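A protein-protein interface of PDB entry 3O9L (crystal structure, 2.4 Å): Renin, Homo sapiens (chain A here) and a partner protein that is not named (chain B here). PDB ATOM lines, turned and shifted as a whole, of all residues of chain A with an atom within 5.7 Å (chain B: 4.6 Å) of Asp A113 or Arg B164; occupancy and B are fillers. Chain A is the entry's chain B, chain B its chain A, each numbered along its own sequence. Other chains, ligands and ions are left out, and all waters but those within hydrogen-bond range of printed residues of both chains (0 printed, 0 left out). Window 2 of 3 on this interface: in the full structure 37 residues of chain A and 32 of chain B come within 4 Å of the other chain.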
ATOM      1  N   SER A   1      16.876  15.033 -11.617  1.00  0.00           N
ATOM      2  CA  SER A   1      16.852  14.423 -10.291  1.00  0.00           C
ATOM      3  C   SER A   1      18.171  14.623  -9.566  1.00  0.00           C
ATOM      4  O   SER A   1      19.236  14.407 -10.142  1.00  0.00           O
ATOM      5  CB  SER A   1      16.546  12.924 -10.394  1.00  0.00           C
ATOM      6  OG  SER A   1      16.625  12.291  -9.124  1.00  0.00           O
ATOM      7  N   LEU A   2      18.083  15.032  -8.302  1.00  0.00           N
ATOM      8  CA  LEU A   2      19.245  15.209  -7.420  1.00  0.00           C
ATOM      9  C   LEU A   2      20.058  13.912  -7.329  1.00  0.00           C
ATOM     10  O   LEU A   2      19.540  12.895  -6.887  1.00  0.00           O
ATOM     11  CB  LEU A   2      18.753  15.619  -6.024  1.00  0.00           C
ATOM     12  CG  LEU A   2      19.725  16.168  -4.977  1.00  0.00           C
ATOM     13  CD1 LEU A   2      19.735  17.698  -5.004  1.00  0.00           C
ATOM     14  CD2 LEU A   2      19.336  15.708  -3.612  1.00  0.00           C
ATOM     15  N   THR A 108      18.308  -4.380   6.150  1.00  0.00           N
ATOM     16  CA  THR A 108      17.852  -5.272   5.070  1.00  0.00           C
ATOM     17  C   THR A 108      17.900  -4.651   3.673  1.00  0.00           C
ATOM     18  O   THR A 108      17.118  -3.749   3.354  1.00  0.00           O
ATOM     19  CB  THR A 108      16.430  -5.843   5.357  1.00  0.00           C
ATOM     20  OG1 THR A 108      16.451  -6.553   6.587  1.00  0.00           O
ATOM     21  CG2 THR A 108      15.947  -6.799   4.246  1.00  0.00           C
ATOM     22  N   LEU A 109      18.807  -5.174   2.849  1.00  0.00           N
ATOM     23  CA  LEU A 109      18.849  -4.869   1.413  1.00  0.00           C
ATOM     24  C   LEU A 109      18.076  -5.933   0.651  1.00  0.00           C
ATOM     25  O   LEU A 109      18.293  -7.126   0.890  1.00  0.00           O
ATOM     26  CB  LEU A 109      20.292  -4.887   0.900  1.00  0.00           C
ATOM     27  CG  LEU A 109      21.269  -3.720   1.029  1.00  0.00           C
ATOM     28  CD1 LEU A 109      22.639  -4.206   0.576  1.00  0.00           C
ATOM     29  CD2 LEU A 109      20.850  -2.536   0.180  1.00  0.00           C
ATOM     30  N   THR A 110      17.198  -5.517  -0.265  1.00  0.00           N
ATOM     31  CA  THR A 110      16.421  -6.465  -1.065  1.00  0.00           C
ATOM     32  C   THR A 110      17.081  -6.727  -2.421  1.00  0.00           C
ATOM     33  O   THR A 110      18.111  -6.125  -2.748  1.00  0.00           O
ATOM     34  CB  THR A 110      14.915  -6.027  -1.266  1.00  0.00           C
ATOM     35  OG1 THR A 110      14.812  -5.059  -2.319  1.00  0.00           O
ATOM     36  CG2 THR A 110      14.298  -5.468   0.030  1.00  0.00           C
ATOM     37  N   SER A 111      16.485  -7.626  -3.202  1.00  0.00           N
ATOM     38  CA  SER A 111      16.908  -7.876  -4.581  1.00  0.00           C
ATOM     39  C   SER A 111      17.052  -6.585  -5.363  1.00  0.00           C
ATOM     40  O   SER A 111      18.034  -6.413  -6.073  1.00  0.00           O
ATOM     41  CB  SER A 111      15.919  -8.787  -5.321  1.00  0.00           C
ATOM     42  OG  SER A 111      16.028  -8.599  -6.735  1.00  0.00           O
ATOM     43  N   ALA A 112      16.056  -5.704  -5.249  1.00  0.00           N
ATOM     44  CA  ALA A 112      16.068  -4.393  -5.945  1.00  0.00           C
ATOM     45  C   ALA A 112      17.191  -3.430  -5.511  1.00  0.00           C
ATOM     46  O   ALA A 112      17.451  -2.447  -6.193  1.00  0.00           O
ATOM     47  CB  ALA A 112      14.712  -3.703  -5.816  1.00  0.00           C
ATOM     48  N   ASP A 113      17.826  -3.690  -4.370  1.00  0.00           N
ATOM     49  CA  ASP A 113      18.855  -2.778  -3.872  1.00  0.00           C
ATOM     50  C   ASP A 113      20.250  -3.249  -4.283  1.00  0.00           C
ATOM     51  O   ASP A 113      21.201  -2.478  -4.226  1.00  0.00           O
ATOM     52  CB  ASP A 113      18.776  -2.610  -2.346  1.00  0.00           C
ATOM     53  CG  ASP A 113      17.430  -2.063  -1.865  1.00  0.00           C
ATOM     54  OD1 ASP A 113      16.891  -1.129  -2.511  1.00  0.00           O
ATOM     55  OD2 ASP A 113      16.922  -2.564  -0.820  1.00  0.00           O
ATOM     56  N   TYR A 114      20.370  -4.505  -4.705  1.00  0.00           N
ATOM     57  CA  TYR A 114      21.681  -5.037  -5.060  1.00  0.00           C
ATOM     58  C   TYR A 114      21.841  -5.695  -6.424  1.00  0.00           C
ATOM     59  O   TYR A 114      22.921  -6.217  -6.715  1.00  0.00           O
ATOM     60  CB  TYR A 114      22.201  -5.943  -3.946  1.00  0.00           C
ATOM     61  CG  TYR A 114      21.606  -7.335  -3.815  1.00  0.00           C
ATOM     62  CD1 TYR A 114      21.926  -8.344  -4.736  1.00  0.00           C
ATOM     63  CD2 TYR A 114      20.801  -7.670  -2.728  1.00  0.00           C
ATOM     64  CE1 TYR A 114      21.425  -9.622  -4.609  1.00  0.00           C
ATOM     65  CE2 TYR A 114      20.290  -8.961  -2.583  1.00  0.00           C
ATOM     66  CZ  TYR A 114      20.614  -9.933  -3.531  1.00  0.00           C
ATOM     67  OH  TYR A 114      20.130 -11.219  -3.431  1.00  0.00           O
ATOM     68  N   VAL A 115      20.788  -5.696  -7.256  1.00  0.00           N
ATOM     69  CA  VAL A 115      20.904  -6.223  -8.633  1.00  0.00           C
ATOM     70  C   VAL A 115      20.619  -5.158  -9.688  1.00  0.00           C
ATOM     71  O   VAL A 115      19.615  -4.441  -9.615  1.00  0.00           O
ATOM     72  CB  VAL A 115      20.028  -7.488  -8.895  1.00  0.00           C
ATOM     73  CG1 VAL A 115      20.235  -8.022 -10.305  1.00  0.00           C
ATOM     74  CG2 VAL A 115      20.377  -8.582  -7.939  1.00  0.00           C
ATOM     75  N   ALA A 129      25.630  -5.684  -7.299  1.00  0.00           N
ATOM     76  CA  ALA A 129      26.363  -4.542  -6.739  1.00  0.00           C
ATOM     77  C   ALA A 129      27.171  -4.940  -5.490  1.00  0.00           C
ATOM     78  O   ALA A 129      27.155  -4.250  -4.471  1.00  0.00           O
ATOM     79  CB  ALA A 129      25.397  -3.402  -6.429  1.00  0.00           C
ATOM     80  N   THR A 148      26.170   1.100  -2.598  1.00  0.00           N
ATOM     81  CA  THR A 148      25.071   0.134  -2.519  1.00  0.00           C
ATOM     82  C   THR A 148      24.319   0.295  -1.200  1.00  0.00           C
ATOM     83  O   THR A 148      23.107   0.497  -1.166  1.00  0.00           O
ATOM     84  CB  THR A 148      25.600  -1.320  -2.624  1.00  0.00           C
ATOM     85  OG1 THR A 148      26.368  -1.473  -3.822  1.00  0.00           O
ATOM     86  CG2 THR A 148      24.437  -2.343  -2.626  1.00  0.00           C
ATOM     87  N   ARG A 151      22.893   4.132  -0.428  1.00  0.00           N
ATOM     88  CA  ARG A 151      21.630   4.435  -1.112  1.00  0.00           C
ATOM     89  C   ARG A 151      20.361   4.158  -0.289  1.00  0.00           C
ATOM     90  O   ARG A 151      19.387   4.902  -0.394  1.00  0.00           O
ATOM     91  CB  ARG A 151      21.532   3.709  -2.453  1.00  0.00           C
ATOM     92  CG  ARG A 151      22.051   4.533  -3.608  1.00  0.00           C
ATOM     93  CD  ARG A 151      21.681   3.952  -4.940  1.00  0.00           C
ATOM     94  NE  ARG A 151      22.252   2.630  -5.095  1.00  0.00           N
ATOM     95  CZ  ARG A 151      23.419   2.350  -5.656  1.00  0.00           C
ATOM     96  NH1 ARG A 151      24.172   3.315  -6.149  1.00  0.00           N
ATOM     97  NH2 ARG A 151      23.820   1.084  -5.729  1.00  0.00           N
ATOM     98  N   LYS A 152      20.376   3.081   0.496  1.00  0.00           N
ATOM     99  CA  LYS A 152      19.220   2.663   1.275  1.00  0.00           C
ATOM    100  C   LYS A 152      19.198   3.283   2.687  1.00  0.00           C
ATOM    101  O   LYS A 152      18.123   3.551   3.256  1.00  0.00           O
ATOM    102  CB  LYS A 152      19.172   1.129   1.351  1.00  0.00           C
ATOM    103  CG  LYS A 152      18.008   0.564   2.181  1.00  0.00           C
ATOM    104  CD  LYS A 152      16.900  -0.012   1.328  1.00  0.00           C
ATOM    105  CE  LYS A 152      16.086  -1.005   2.140  1.00  0.00           C
ATOM    106  NZ  LYS A 152      15.309  -1.974   1.283  1.00  0.00           N
ATOM    107  N   HIS A 171      13.322   8.759  -1.038  1.00  0.00           N
ATOM    108  CA  HIS A 171      13.601   9.158  -2.416  1.00  0.00           C
ATOM    109  C   HIS A 171      12.431   9.906  -3.065  1.00  0.00           C
ATOM    110  O   HIS A 171      12.587  10.607  -4.071  1.00  0.00           O
ATOM    111  CB  HIS A 171      14.054   7.947  -3.247  1.00  0.00           C
ATOM    112  CG  HIS A 171      15.313   7.307  -2.738  1.00  0.00           C
ATOM    113  ND1 HIS A 171      15.426   5.949  -2.518  1.00  0.00           N
ATOM    114  CD2 HIS A 171      16.509   7.844  -2.395  1.00  0.00           C
ATOM    115  CE1 HIS A 171      16.641   5.678  -2.071  1.00  0.00           C
ATOM    116  NE2 HIS A 171      17.319   6.810  -1.991  1.00  0.00           N
ATOM    117  N   ASN B  14      25.196  11.792  -9.725  1.00  0.00           N
ATOM    118  CA  ASN B  14      25.196  10.326  -9.732  1.00  0.00           C
ATOM    119  C   ASN B  14      25.448   9.800 -11.131  1.00  0.00           C
ATOM    120  O   ASN B  14      24.561   9.802 -11.981  1.00  0.00           O
ATOM    121  CB  ASN B  14      23.875   9.755  -9.172  1.00  0.00           C
ATOM    122  CG  ASN B  14      23.702   8.220  -9.424  1.00  0.00           C
ATOM    123  OD1 ASN B  14      24.429   7.589 -10.196  1.00  0.00           O
ATOM    124  ND2 ASN B  14      22.731   7.642  -8.753  1.00  0.00           N
ATOM    125  N   ASP B  17      24.805   4.916 -10.733  1.00  0.00           N
ATOM    126  CA  ASP B  17      24.866   4.241  -9.424  1.00  0.00           C
ATOM    127  C   ASP B  17      26.271   3.780  -8.949  1.00  0.00           C
ATOM    128  O   ASP B  17      26.374   3.111  -7.911  1.00  0.00           O
ATOM    129  CB  ASP B  17      23.882   3.059  -9.349  1.00  0.00           C
ATOM    130  CG  ASP B  17      22.402   3.485  -9.374  1.00  0.00           C
ATOM    131  OD1 ASP B  17      22.068   4.680  -9.137  1.00  0.00           O
ATOM    132  OD2 ASP B  17      21.567   2.584  -9.620  1.00  0.00           O
ATOM    133  N   TYR B 162      22.806   9.638  -1.108  1.00  0.00           N
ATOM    134  CA  TYR B 162      23.004   9.130  -2.466  1.00  0.00           C
ATOM    135  C   TYR B 162      21.661   8.640  -3.071  1.00  0.00           C
ATOM    136  O   TYR B 162      21.042   7.698  -2.544  1.00  0.00           O
ATOM    137  CB  TYR B 162      23.958   7.914  -2.453  1.00  0.00           C
ATOM    138  CG  TYR B 162      25.445   8.163  -2.231  1.00  0.00           C
ATOM    139  CD1 TYR B 162      25.968   9.466  -2.115  1.00  0.00           C
ATOM    140  CD2 TYR B 162      26.341   7.085  -2.191  1.00  0.00           C
ATOM    141  CE1 TYR B 162      27.359   9.692  -1.935  1.00  0.00           C
ATOM    142  CE2 TYR B 162      27.724   7.287  -2.002  1.00  0.00           C
ATOM    143  CZ  TYR B 162      28.228   8.602  -1.870  1.00  0.00           C
ATOM    144  OH  TYR B 162      29.584   8.820  -1.675  1.00  0.00           O
ATOM    145  N   ASN B 163      21.235   9.232  -4.184  1.00  0.00           N
ATOM    146  CA  ASN B 163      20.010   8.820  -4.875  1.00  0.00           C
ATOM    147  C   ASN B 163      20.164   7.485  -5.654  1.00  0.00           C
ATOM    148  O   ASN B 163      21.264   6.920  -5.736  1.00  0.00           O
ATOM    149  CB  ASN B 163      19.535   9.944  -5.811  1.00  0.00           C
ATOM    150  CG  ASN B 163      17.999  10.041  -5.906  1.00  0.00           C
ATOM    151  OD1 ASN B 163      17.319   9.150  -6.442  1.00  0.00           O
ATOM    152  ND2 ASN B 163      17.452  11.145  -5.387  1.00  0.00           N
ATOM    153  N   ARG B 164      19.053   6.981  -6.195  1.00  0.00           N
ATOM    154  CA  ARG B 164      19.066   5.877  -7.168  1.00  0.00           C
ATOM    155  C   ARG B 164      19.079   6.463  -8.577  1.00  0.00           C
ATOM    156  O   ARG B 164      19.160   7.684  -8.735  1.00  0.00           O
ATOM    157  CB  ARG B 164      17.844   4.963  -6.992  1.00  0.00           C
ATOM    158  CG  ARG B 164      17.715   4.343  -5.607  1.00  0.00           C
ATOM    159  CD  ARG B 164      16.699   3.207  -5.569  1.00  0.00           C
ATOM    160  NE  ARG B 164      16.195   3.005  -4.204  1.00  0.00           N
ATOM    161  CZ  ARG B 164      16.774   2.252  -3.266  1.00  0.00           C
ATOM    162  NH1 ARG B 164      17.898   1.587  -3.515  1.00  0.00           N
ATOM    163  NH2 ARG B 164      16.216   2.159  -2.061  1.00  0.00           N
ATOM    164  N   ASP B 165      18.985   5.608  -9.594  1.00  0.00           N
ATOM    165  CA  ASP B 165      19.037   6.050 -10.995  1.00  0.00           C
ATOM    166  C   ASP B 165      17.727   5.752 -11.756  1.00  0.00           C
ATOM    167  O   ASP B 165      17.602   6.004 -12.972  1.00  0.00           O
ATOM    168  CB  ASP B 165      20.232   5.402 -11.706  1.00  0.00           C
ATOM    169  CG  ASP B 165      20.822   6.289 -12.791  1.00  0.00           C
ATOM    170  OD1 ASP B 165      21.362   7.362 -12.452  1.00  0.00           O
ATOM    171  OD2 ASP B 165      20.756   5.908 -13.984  1.00  0.00           O
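Of the printed residues of chain B, Ser A1 touches Asn B163 (3.995 Å).
Of the printed residues of chain B, Leu A2 touches Asn B163 (3.1 Å).
Of the printed residues of chain B, His A171 touches Tyr B162 and Arg B164.
Of the printed residues of chain B, Arg A151 touches Asp B17 (2.8 Å), Tyr B162 (3.5 Å), Asn B163 (3.1 Å) and Arg B164 (3.9 Å).
Val A115 touches none of the printed residues of chain B.
Thr A148 touches none of the printed residues of chain B.
The nearest printed residue of chain B that does not touch Asp A113 is Asp B17 (7.4 Å).
The nearest printed residue of chain A that does not touch Asp B17 is Thr A148 (5.7 Å).
Of the 6 printed residues of chain B, 4 touch a printed residue of chain A.
Along chain B the printed residues that touch a printed residue of chain A span positions 17 to 164.
Printed residues of chain A that touch a printed residue of chain B: Ser A1, Leu A2, Asp A113, Arg A151 and His A171.
Hydrophobic or aromatic side chains of chain A that line the printed part of chain B: His A171.
Among the printed residues, 9 pairs touch across the chains.
Among the printed residues, Asp or Glu carboxylates within 4 Å of a Lys or Arg side-chain nitrogen of the other chain: Asp A113 with Arg B164 and Arg A151 with Asp B17.
Among the printed residues, merely in contact across the chains: Arg A151 with Asn B163 (3.1 Å), Arg A151 with Tyr B162 (3.5 Å), His A171 with Tyr B162 (3.9 Å), Arg A151 with Arg B164 (3.9 Å) and Ser A1 with Asn B163 (3.995 Å).
The side-chain amide nitrogen (ND2) of Asn B163 lies within hydrogen-bond range of the backbone carbonyl oxygen (O) of Leu A2 (3.1 Å).
The guanidinium group (NE) of Arg B164 sits close to a ring nitrogen (ND1) of His A171, at 3.5 Å.
The guanidinium group (NH1) of Arg B164 is in salt-bridge range of the side-chain carboxylate (OD1) of Asp A113 (3.1 Å).
OD1 of Asp B17 is in salt-bridge range of NH1 of Arg A151.
The side-chain carboxylate (OD1) of Asp B17 sits close to the backbone NH (N) of Asp B165.
O of Arg A151 is in hydrogen-bond range of NE2 of His A171 (3.2 Å).
OD2 of Asp A113 lies within hydrogen-bond range of N of Thr A110.
The backbone NH (N) of Asp B17 sits at hydrogen-bond distance from the side-chain amide oxygen (OD1) of Asn B14 (2.8 Å).
The side-chain amide nitrogen (ND2) of Asn B14 sits at hydrogen-bond distance from the backbone carbonyl oxygen (O) of Asn B163 (3.4 Å).
OD2 of Asp A113 is in salt-bridge range of NZ of Lys A152.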
